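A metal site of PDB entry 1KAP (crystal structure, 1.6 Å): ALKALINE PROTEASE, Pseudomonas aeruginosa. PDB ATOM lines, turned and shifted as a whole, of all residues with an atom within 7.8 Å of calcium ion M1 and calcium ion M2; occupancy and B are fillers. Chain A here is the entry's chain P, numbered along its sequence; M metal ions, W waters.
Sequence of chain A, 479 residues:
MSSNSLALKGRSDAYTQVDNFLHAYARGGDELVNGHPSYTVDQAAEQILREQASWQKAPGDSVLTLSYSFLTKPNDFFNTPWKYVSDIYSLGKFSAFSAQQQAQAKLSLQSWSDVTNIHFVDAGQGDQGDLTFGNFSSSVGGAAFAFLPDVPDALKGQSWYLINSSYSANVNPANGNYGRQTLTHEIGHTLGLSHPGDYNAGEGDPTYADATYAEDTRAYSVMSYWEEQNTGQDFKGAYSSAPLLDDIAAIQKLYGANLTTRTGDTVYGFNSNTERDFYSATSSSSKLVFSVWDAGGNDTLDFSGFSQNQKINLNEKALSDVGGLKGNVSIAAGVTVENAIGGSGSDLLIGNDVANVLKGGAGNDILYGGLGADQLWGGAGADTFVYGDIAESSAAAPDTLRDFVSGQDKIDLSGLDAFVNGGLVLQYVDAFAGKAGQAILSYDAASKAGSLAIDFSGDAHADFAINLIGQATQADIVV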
ATOM      1  N   THR A 261      -9.909   1.020   5.171  1.00  0.00           N
ATOM      2  CA  THR A 261     -10.395   1.313   3.826  1.00  0.00           C
ATOM      3  C   THR A 261     -10.657   2.791   3.529  1.00  0.00           C
ATOM      4  O   THR A 261     -11.402   3.449   4.259  1.00  0.00           O
ATOM      5  CB  THR A 261     -11.669   0.497   3.550  1.00  0.00           C
ATOM      6  OG1 THR A 261     -11.337  -0.893   3.660  1.00  0.00           O
ATOM      7  CG2 THR A 261     -12.224   0.789   2.157  1.00  0.00           C
ATOM      8  N   ARG A 262     -10.032   3.297   2.474  1.00  0.00           N
ATOM      9  CA  ARG A 262     -10.199   4.683   2.030  1.00  0.00           C
ATOM     10  C   ARG A 262     -10.036   5.697   3.150  1.00  0.00           C
ATOM     11  O   ARG A 262     -10.872   6.578   3.339  1.00  0.00           O
ATOM     12  CB  ARG A 262     -11.570   4.841   1.329  1.00  0.00           C
ATOM     13  CG  ARG A 262     -11.644   4.098  -0.023  1.00  0.00           C
ATOM     14  CD  ARG A 262     -13.034   4.131  -0.692  1.00  0.00           C
ATOM     15  NE  ARG A 262     -14.036   3.325   0.012  1.00  0.00           N
ATOM     16  CZ  ARG A 262     -14.261   2.031  -0.223  1.00  0.00           C
ATOM     17  NH1 ARG A 262     -13.555   1.367  -1.133  1.00  0.00           N
ATOM     18  NH2 ARG A 262     -15.238   1.396   0.433  1.00  0.00           N
ATOM     19  N   THR A 263      -8.957   5.559   3.936  1.00  0.00           N
ATOM     20  CA  THR A 263      -8.701   6.479   5.047  1.00  0.00           C
ATOM     21  C   THR A 263      -8.221   7.863   4.601  1.00  0.00           C
ATOM     22  O   THR A 263      -8.124   8.766   5.422  1.00  0.00           O
ATOM     23  CB  THR A 263      -7.695   5.901   6.099  1.00  0.00           C
ATOM     24  OG1 THR A 263      -6.494   5.475   5.455  1.00  0.00           O
ATOM     25  CG2 THR A 263      -8.315   4.779   6.862  1.00  0.00           C
ATOM     26  N   GLY A 264      -7.870   8.010   3.326  1.00  0.00           N
ATOM     27  CA  GLY A 264      -7.453   9.319   2.827  1.00  0.00           C
ATOM     28  C   GLY A 264      -8.684  10.155   2.491  1.00  0.00           C
ATOM     29  O   GLY A 264      -9.806   9.751   2.783  1.00  0.00           O
ATOM     30  N   ASP A 265      -8.493  11.322   1.897  1.00  0.00           N
ATOM     31  CA  ASP A 265      -9.621  12.190   1.521  1.00  0.00           C
ATOM     32  C   ASP A 265     -10.185  11.551   0.269  1.00  0.00           C
ATOM     33  O   ASP A 265      -9.504  11.448  -0.750  1.00  0.00           O
ATOM     34  CB  ASP A 265      -9.148  13.615   1.250  1.00  0.00           C
ATOM     35  CG  ASP A 265      -8.521  14.277   2.483  1.00  0.00           C
ATOM     36  OD1 ASP A 265      -8.719  13.796   3.617  1.00  0.00           O
ATOM     37  OD2 ASP A 265      -7.824  15.282   2.311  1.00  0.00           O
ATOM     38  N   THR A 266     -11.461  11.178   0.319  1.00  0.00           N
ATOM     39  CA  THR A 266     -12.064  10.435  -0.785  1.00  0.00           C
ATOM     40  C   THR A 266     -13.239  11.117  -1.446  1.00  0.00           C
ATOM     41  O   THR A 266     -14.092  11.678  -0.773  1.00  0.00           O
ATOM     42  CB  THR A 266     -12.560   9.054  -0.241  1.00  0.00           C
ATOM     43  OG1 THR A 266     -11.606   8.521   0.682  1.00  0.00           O
ATOM     44  CG2 THR A 266     -12.771   8.071  -1.389  1.00  0.00           C
ATOM     45  N   VAL A 267     -13.303  11.012  -2.775  1.00  0.00           N
ATOM     46  CA  VAL A 267     -14.406  11.564  -3.552  1.00  0.00           C
ATOM     47  C   VAL A 267     -15.189  10.417  -4.188  1.00  0.00           C
ATOM     48  O   VAL A 267     -14.619   9.522  -4.828  1.00  0.00           O
ATOM     49  CB  VAL A 267     -13.904  12.475  -4.698  1.00  0.00           C
ATOM     50  CG1 VAL A 267     -15.085  13.009  -5.496  1.00  0.00           C
ATOM     51  CG2 VAL A 267     -13.071  13.613  -4.133  1.00  0.00           C
ATOM     52  N   TYR A 268     -16.501  10.428  -3.968  1.00  0.00           N
ATOM     53  CA  TYR A 268     -17.424   9.442  -4.504  1.00  0.00           C
ATOM     54  C   TYR A 268     -18.278  10.126  -5.563  1.00  0.00           C
ATOM     55  O   TYR A 268     -18.682  11.286  -5.386  1.00  0.00           O
ATOM     56  CB  TYR A 268     -18.337   8.904  -3.404  1.00  0.00           C
ATOM     57  CG  TYR A 268     -17.603   8.162  -2.313  1.00  0.00           C
ATOM     58  CD1 TYR A 268     -17.053   8.844  -1.215  1.00  0.00           C
ATOM     59  CD2 TYR A 268     -17.372   6.780  -2.415  1.00  0.00           C
ATOM     60  CE1 TYR A 268     -16.291   8.176  -0.238  1.00  0.00           C
ATOM     61  CE2 TYR A 268     -16.625   6.096  -1.443  1.00  0.00           C
ATOM     62  CZ  TYR A 268     -16.083   6.808  -0.365  1.00  0.00           C
ATOM     63  OH  TYR A 268     -15.297   6.155   0.552  1.00  0.00           O
ATOM     64  N   ASN A 273     -11.814   9.096  -6.713  1.00  0.00           N
ATOM     65  CA  ASN A 273     -10.448   8.598  -6.514  1.00  0.00           C
ATOM     66  C   ASN A 273     -10.540   7.275  -5.750  1.00  0.00           C
ATOM     67  O   ASN A 273      -9.577   6.858  -5.116  1.00  0.00           O
ATOM     68  CB  ASN A 273      -9.551   9.622  -5.782  1.00  0.00           C
ATOM     69  CG  ASN A 273     -10.025   9.911  -4.364  1.00  0.00           C
ATOM     70  OD1 ASN A 273     -11.164   9.642  -4.012  1.00  0.00           O
ATOM     71  ND2 ASN A 273      -9.134  10.444  -3.549  1.00  0.00           N
ATOM     72  N   VAL A 292     -21.862   3.970   0.918  1.00  0.00           N
ATOM     73  CA  VAL A 292     -20.502   4.381   1.246  1.00  0.00           C
ATOM     74  C   VAL A 292     -19.906   3.795   2.521  1.00  0.00           C
ATOM     75  O   VAL A 292     -20.488   3.941   3.600  1.00  0.00           O
ATOM     76  CB  VAL A 292     -20.409   5.944   1.353  1.00  0.00           C
ATOM     77  CG1 VAL A 292     -18.982   6.398   1.733  1.00  0.00           C
ATOM     78  CG2 VAL A 292     -20.890   6.606   0.063  1.00  0.00           C
ATOM     79  N   TRP A 293     -18.782   3.099   2.383  1.00  0.00           N
ATOM     80  CA  TRP A 293     -18.040   2.610   3.553  1.00  0.00           C
ATOM     81  C   TRP A 293     -16.726   3.371   3.413  1.00  0.00           C
ATOM     82  O   TRP A 293     -16.080   3.316   2.371  1.00  0.00           O
ATOM     83  CB  TRP A 293     -17.764   1.101   3.572  1.00  0.00           C
ATOM     84  CG  TRP A 293     -16.855   0.755   4.714  1.00  0.00           C
ATOM     85  CD1 TRP A 293     -15.536   0.393   4.635  1.00  0.00           C
ATOM     86  CD2 TRP A 293     -17.125   0.935   6.119  1.00  0.00           C
ATOM     87  NE1 TRP A 293     -14.974   0.363   5.886  1.00  0.00           N
ATOM     88  CE2 TRP A 293     -15.916   0.688   6.813  1.00  0.00           C
ATOM     89  CE3 TRP A 293     -18.277   1.292   6.841  1.00  0.00           C
ATOM     90  CZ2 TRP A 293     -15.820   0.793   8.214  1.00  0.00           C
ATOM     91  CZ3 TRP A 293     -18.179   1.406   8.246  1.00  0.00           C
ATOM     92  CH2 TRP A 293     -16.954   1.156   8.906  1.00  0.00           C
ATOM     93  N   ASP A 294     -16.340   4.099   4.456  1.00  0.00           N
ATOM     94  CA  ASP A 294     -15.132   4.929   4.413  1.00  0.00           C
ATOM     95  C   ASP A 294     -14.657   5.048   5.862  1.00  0.00           C
ATOM     96  O   ASP A 294     -15.441   5.372   6.744  1.00  0.00           O
ATOM     97  CB  ASP A 294     -15.499   6.304   3.822  1.00  0.00           C
ATOM     98  CG  ASP A 294     -14.282   7.176   3.581  1.00  0.00           C
ATOM     99  OD1 ASP A 294     -13.614   7.530   4.575  1.00  0.00           O
ATOM    100  OD2 ASP A 294     -14.014   7.512   2.411  1.00  0.00           O
ATOM    101  N   ALA A 295     -13.382   4.757   6.088  1.00  0.00           N
ATOM    102  CA  ALA A 295     -12.830   4.748   7.443  1.00  0.00           C
ATOM    103  C   ALA A 295     -12.166   6.017   7.962  1.00  0.00           C
ATOM    104  O   ALA A 295     -11.748   6.064   9.113  1.00  0.00           O
ATOM    105  CB  ALA A 295     -11.877   3.562   7.604  1.00  0.00           C
ATOM    106  N   GLY A 296     -12.018   7.040   7.119  1.00  0.00           N
ATOM    107  CA  GLY A 296     -11.408   8.270   7.597  1.00  0.00           C
ATOM    108  C   GLY A 296     -11.142   9.289   6.519  1.00  0.00           C
ATOM    109  O   GLY A 296     -11.348   9.013   5.354  1.00  0.00           O
ATOM    110  N   GLY A 297     -10.697  10.482   6.902  1.00  0.00           N
ATOM    111  CA  GLY A 297     -10.384  11.509   5.929  1.00  0.00           C
ATOM    112  C   GLY A 297     -11.519  12.472   5.662  1.00  0.00           C
ATOM    113  O   GLY A 297     -12.612  12.341   6.218  1.00  0.00           O
ATOM    114  N   ASN A 298     -11.237  13.477   4.844  1.00  0.00           N
ATOM    115  CA  ASN A 298     -12.204  14.507   4.448  1.00  0.00           C
ATOM    116  C   ASN A 298     -12.769  14.033   3.126  1.00  0.00           C
ATOM    117  O   ASN A 298     -12.093  14.075   2.095  1.00  0.00           O
ATOM    118  CB  ASN A 298     -11.491  15.856   4.300  1.00  0.00           C
ATOM    119  CG  ASN A 298     -12.457  16.974   3.934  1.00  0.00           C
ATOM    120  OD1 ASN A 298     -13.494  17.138   4.568  1.00  0.00           O
ATOM    121  ND2 ASN A 298     -12.120  17.732   2.907  1.00  0.00           N
ATOM    122  N   ASP A 299     -14.023  13.629   3.153  1.00  0.00           N
ATOM    123  CA  ASP A 299     -14.688  13.023   2.006  1.00  0.00           C
ATOM    124  C   ASP A 299     -15.805  13.836   1.365  1.00  0.00           C
ATOM    125  O   ASP A 299     -16.520  14.578   2.048  1.00  0.00           O
ATOM    126  CB  ASP A 299     -15.200  11.654   2.428  1.00  0.00           C
ATOM    127  CG  ASP A 299     -14.172  10.891   3.243  1.00  0.00           C
ATOM    128  OD1 ASP A 299     -13.079  10.630   2.698  1.00  0.00           O
ATOM    129  OD2 ASP A 299     -14.420  10.603   4.417  1.00  0.00           O
ATOM    130  N   THR A 300     -16.033  13.579   0.092  1.00  0.00           N
ATOM    131  CA  THR A 300     -17.005  14.335  -0.677  1.00  0.00           C
ATOM    132  C   THR A 300     -17.867  13.484  -1.596  1.00  0.00           C
ATOM    133  O   THR A 300     -17.368  12.557  -2.251  1.00  0.00           O
ATOM    134  CB  THR A 300     -16.249  15.331  -1.612  1.00  0.00           C
ATOM    135  OG1 THR A 300     -15.405  16.185  -0.819  1.00  0.00           O
ATOM    136  CG2 THR A 300     -17.222  16.183  -2.443  1.00  0.00           C
ATOM    137  N   VAL A 335     -20.132   5.884   9.456  1.00  0.00           N
ATOM    138  CA  VAL A 335     -19.320   6.597   8.490  1.00  0.00           C
ATOM    139  C   VAL A 335     -19.626   8.095   8.490  1.00  0.00           C
ATOM    140  O   VAL A 335     -20.797   8.493   8.484  1.00  0.00           O
ATOM    141  CB  VAL A 335     -19.564   6.046   7.072  1.00  0.00           C
ATOM    142  CG1 VAL A 335     -18.858   6.915   6.032  1.00  0.00           C
ATOM    143  CG2 VAL A 335     -19.071   4.612   7.004  1.00  0.00           C
ATOM    144  N   THR A 336     -18.577   8.913   8.499  1.00  0.00           N
ATOM    145  CA  THR A 336     -18.754  10.361   8.461  1.00  0.00           C
ATOM    146  C   THR A 336     -18.262  10.925   7.129  1.00  0.00           C
ATOM    147  O   THR A 336     -17.066  10.900   6.839  1.00  0.00           O
ATOM    148  CB  THR A 336     -18.030  11.094   9.637  1.00  0.00           C
ATOM    149  OG1 THR A 336     -18.489  10.549  10.887  1.00  0.00           O
ATOM    150  CG2 THR A 336     -18.297  12.604   9.606  1.00  0.00           C
ATOM    151  N   VAL A 337     -19.205  11.376   6.314  1.00  0.00           N
ATOM    152  CA  VAL A 337     -18.910  12.005   5.022  1.00  0.00           C
ATOM    153  C   VAL A 337     -19.115  13.515   5.274  1.00  0.00           C
ATOM    154  O   VAL A 337     -20.150  13.926   5.814  1.00  0.00           O
ATOM    155  CB  VAL A 337     -19.823  11.478   3.913  1.00  0.00           C
ATOM    156  CG1 VAL A 337     -19.513  12.208   2.602  1.00  0.00           C
ATOM    157  CG2 VAL A 337     -19.586   9.966   3.744  1.00  0.00           C
ATOM    158  N   GLU A 338     -18.137  14.299   4.851  1.00  0.00           N
ATOM    159  CA  GLU A 338     -18.125  15.723   5.139  1.00  0.00           C
ATOM    160  C   GLU A 338     -18.725  16.708   4.164  1.00  0.00           C
ATOM    161  O   GLU A 338     -19.344  17.690   4.573  1.00  0.00           O
ATOM    162  CB  GLU A 338     -16.682  16.170   5.431  1.00  0.00           C
ATOM    163  CG  GLU A 338     -16.042  15.607   6.700  1.00  0.00           C
ATOM    164  CD  GLU A 338     -15.639  14.129   6.634  1.00  0.00           C
ATOM    165  OE1 GLU A 338     -15.577  13.530   5.535  1.00  0.00           O
ATOM    166  OE2 GLU A 338     -15.369  13.557   7.708  1.00  0.00           O
ATOM    167  N   ASN A 339     -18.544  16.458   2.870  1.00  0.00           N
ATOM    168  CA  ASN A 339     -18.977  17.424   1.864  1.00  0.00           C
ATOM    169  C   ASN A 339     -19.865  16.838   0.785  1.00  0.00           C
ATOM    170  O   ASN A 339     -19.857  15.638   0.554  1.00  0.00           O
ATOM    171  CB  ASN A 339     -17.713  18.006   1.197  1.00  0.00           C
ATOM    172  CG  ASN A 339     -16.639  18.322   2.208  1.00  0.00           C
ATOM    173  OD1 ASN A 339     -16.874  19.040   3.172  1.00  0.00           O
ATOM    174  ND2 ASN A 339     -15.461  17.722   2.036  1.00  0.00           N
ATOM    175  N   VAL A 354     -21.218  17.460  11.701  1.00  0.00           N
ATOM    176  CA  VAL A 354     -19.886  18.042  11.635  1.00  0.00           C
ATOM    177  C   VAL A 354     -19.864  19.213  10.663  1.00  0.00           C
ATOM    178  O   VAL A 354     -20.865  19.496  10.006  1.00  0.00           O
ATOM    179  CB  VAL A 354     -18.785  16.982  11.243  1.00  0.00           C
ATOM    180  CG1 VAL A 354     -18.838  15.804  12.226  1.00  0.00           C
ATOM    181  CG2 VAL A 354     -18.940  16.498   9.788  1.00  0.00           C
HETATM  182 CA    CA M   1     -14.746  11.386   6.614  1.00  0.00          CA
HETATM  183 CA    CA M   2     -11.943   8.665   3.122  1.00  0.00          CA
HETATM  184  O   HOH W   1     -14.534   8.964   6.731  1.00  0.00           O
HETATM  185  O   HOH W   2     -14.114  11.052   8.921  1.00  0.00           O
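Calcium ion M2 is bound by OD1 of Asp 299 (2.3 Å), O of Gly 296 (2.3 Å), O of Arg 262 (2.4 Å), O of Gly 264 (2.4 Å), OG1 of Thr 266 (2.5 Å), OD2 of Asp 294 (2.5 Å) and OD1 of Asp 294 (2.5 Å).
Of the 24 residues printed, 6 come within 4 Å of calcium ion M2. The nearest printed residue that does not touch calcium ion M2 is Thr 263 (4.1 Å).
The side-chain carboxylate (OD2) of Asp 299 binds calcium ion M1 (2.4 Å). O of Gly 297 binds calcium ion M1 (2.4 Å). Calcium ion M1 is bound by O of Thr 336 (2.4 Å). Water W2 is bound to calcium ion M1, 2.4 Å away. Water W1 is bound to calcium ion M1, 2.4 Å away. Calcium ion M1 is bound by OE2 of Glu 338 (2.5 Å). OE1 of Glu 338 is bound to calcium ion M1.
Four residues have an atom within 4 Å of calcium ion M1: Gly 297, Asp 299, Thr 336 and Glu 338. The nearest printed residue that does not touch calcium ion M1 is Gly 296 (4.2 Å).
The backbone NH of Asn 339 lies within hydrogen-bond range of the backbone carbonyl oxygen of Asp 299 (2.9 Å). The side-chain hydroxyl (OH) of Tyr 268 lies within hydrogen-bond range of the guanidinium group (NE) of Arg 262. The guanidinium group of Arg 262 sits at hydrogen-bond distance from the backbone carbonyl oxygen of Trp 293 (2.9 Å). The backbone NH of Gly 297 sits at hydrogen-bond distance from the backbone carbonyl oxygen of Thr 263 (3.4 Å). The backbone NH of Thr 266 is in hydrogen-bond range of the backbone carbonyl oxygen of Asn 298, 3.5 Å away. The backbone carbonyl oxygen of Thr 266 sits at hydrogen-bond distance from the backbone NH of Thr 300 (2.9 Å). OD2 of Asp 294 sits close to OH of Tyr 268 (2.6 Å).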
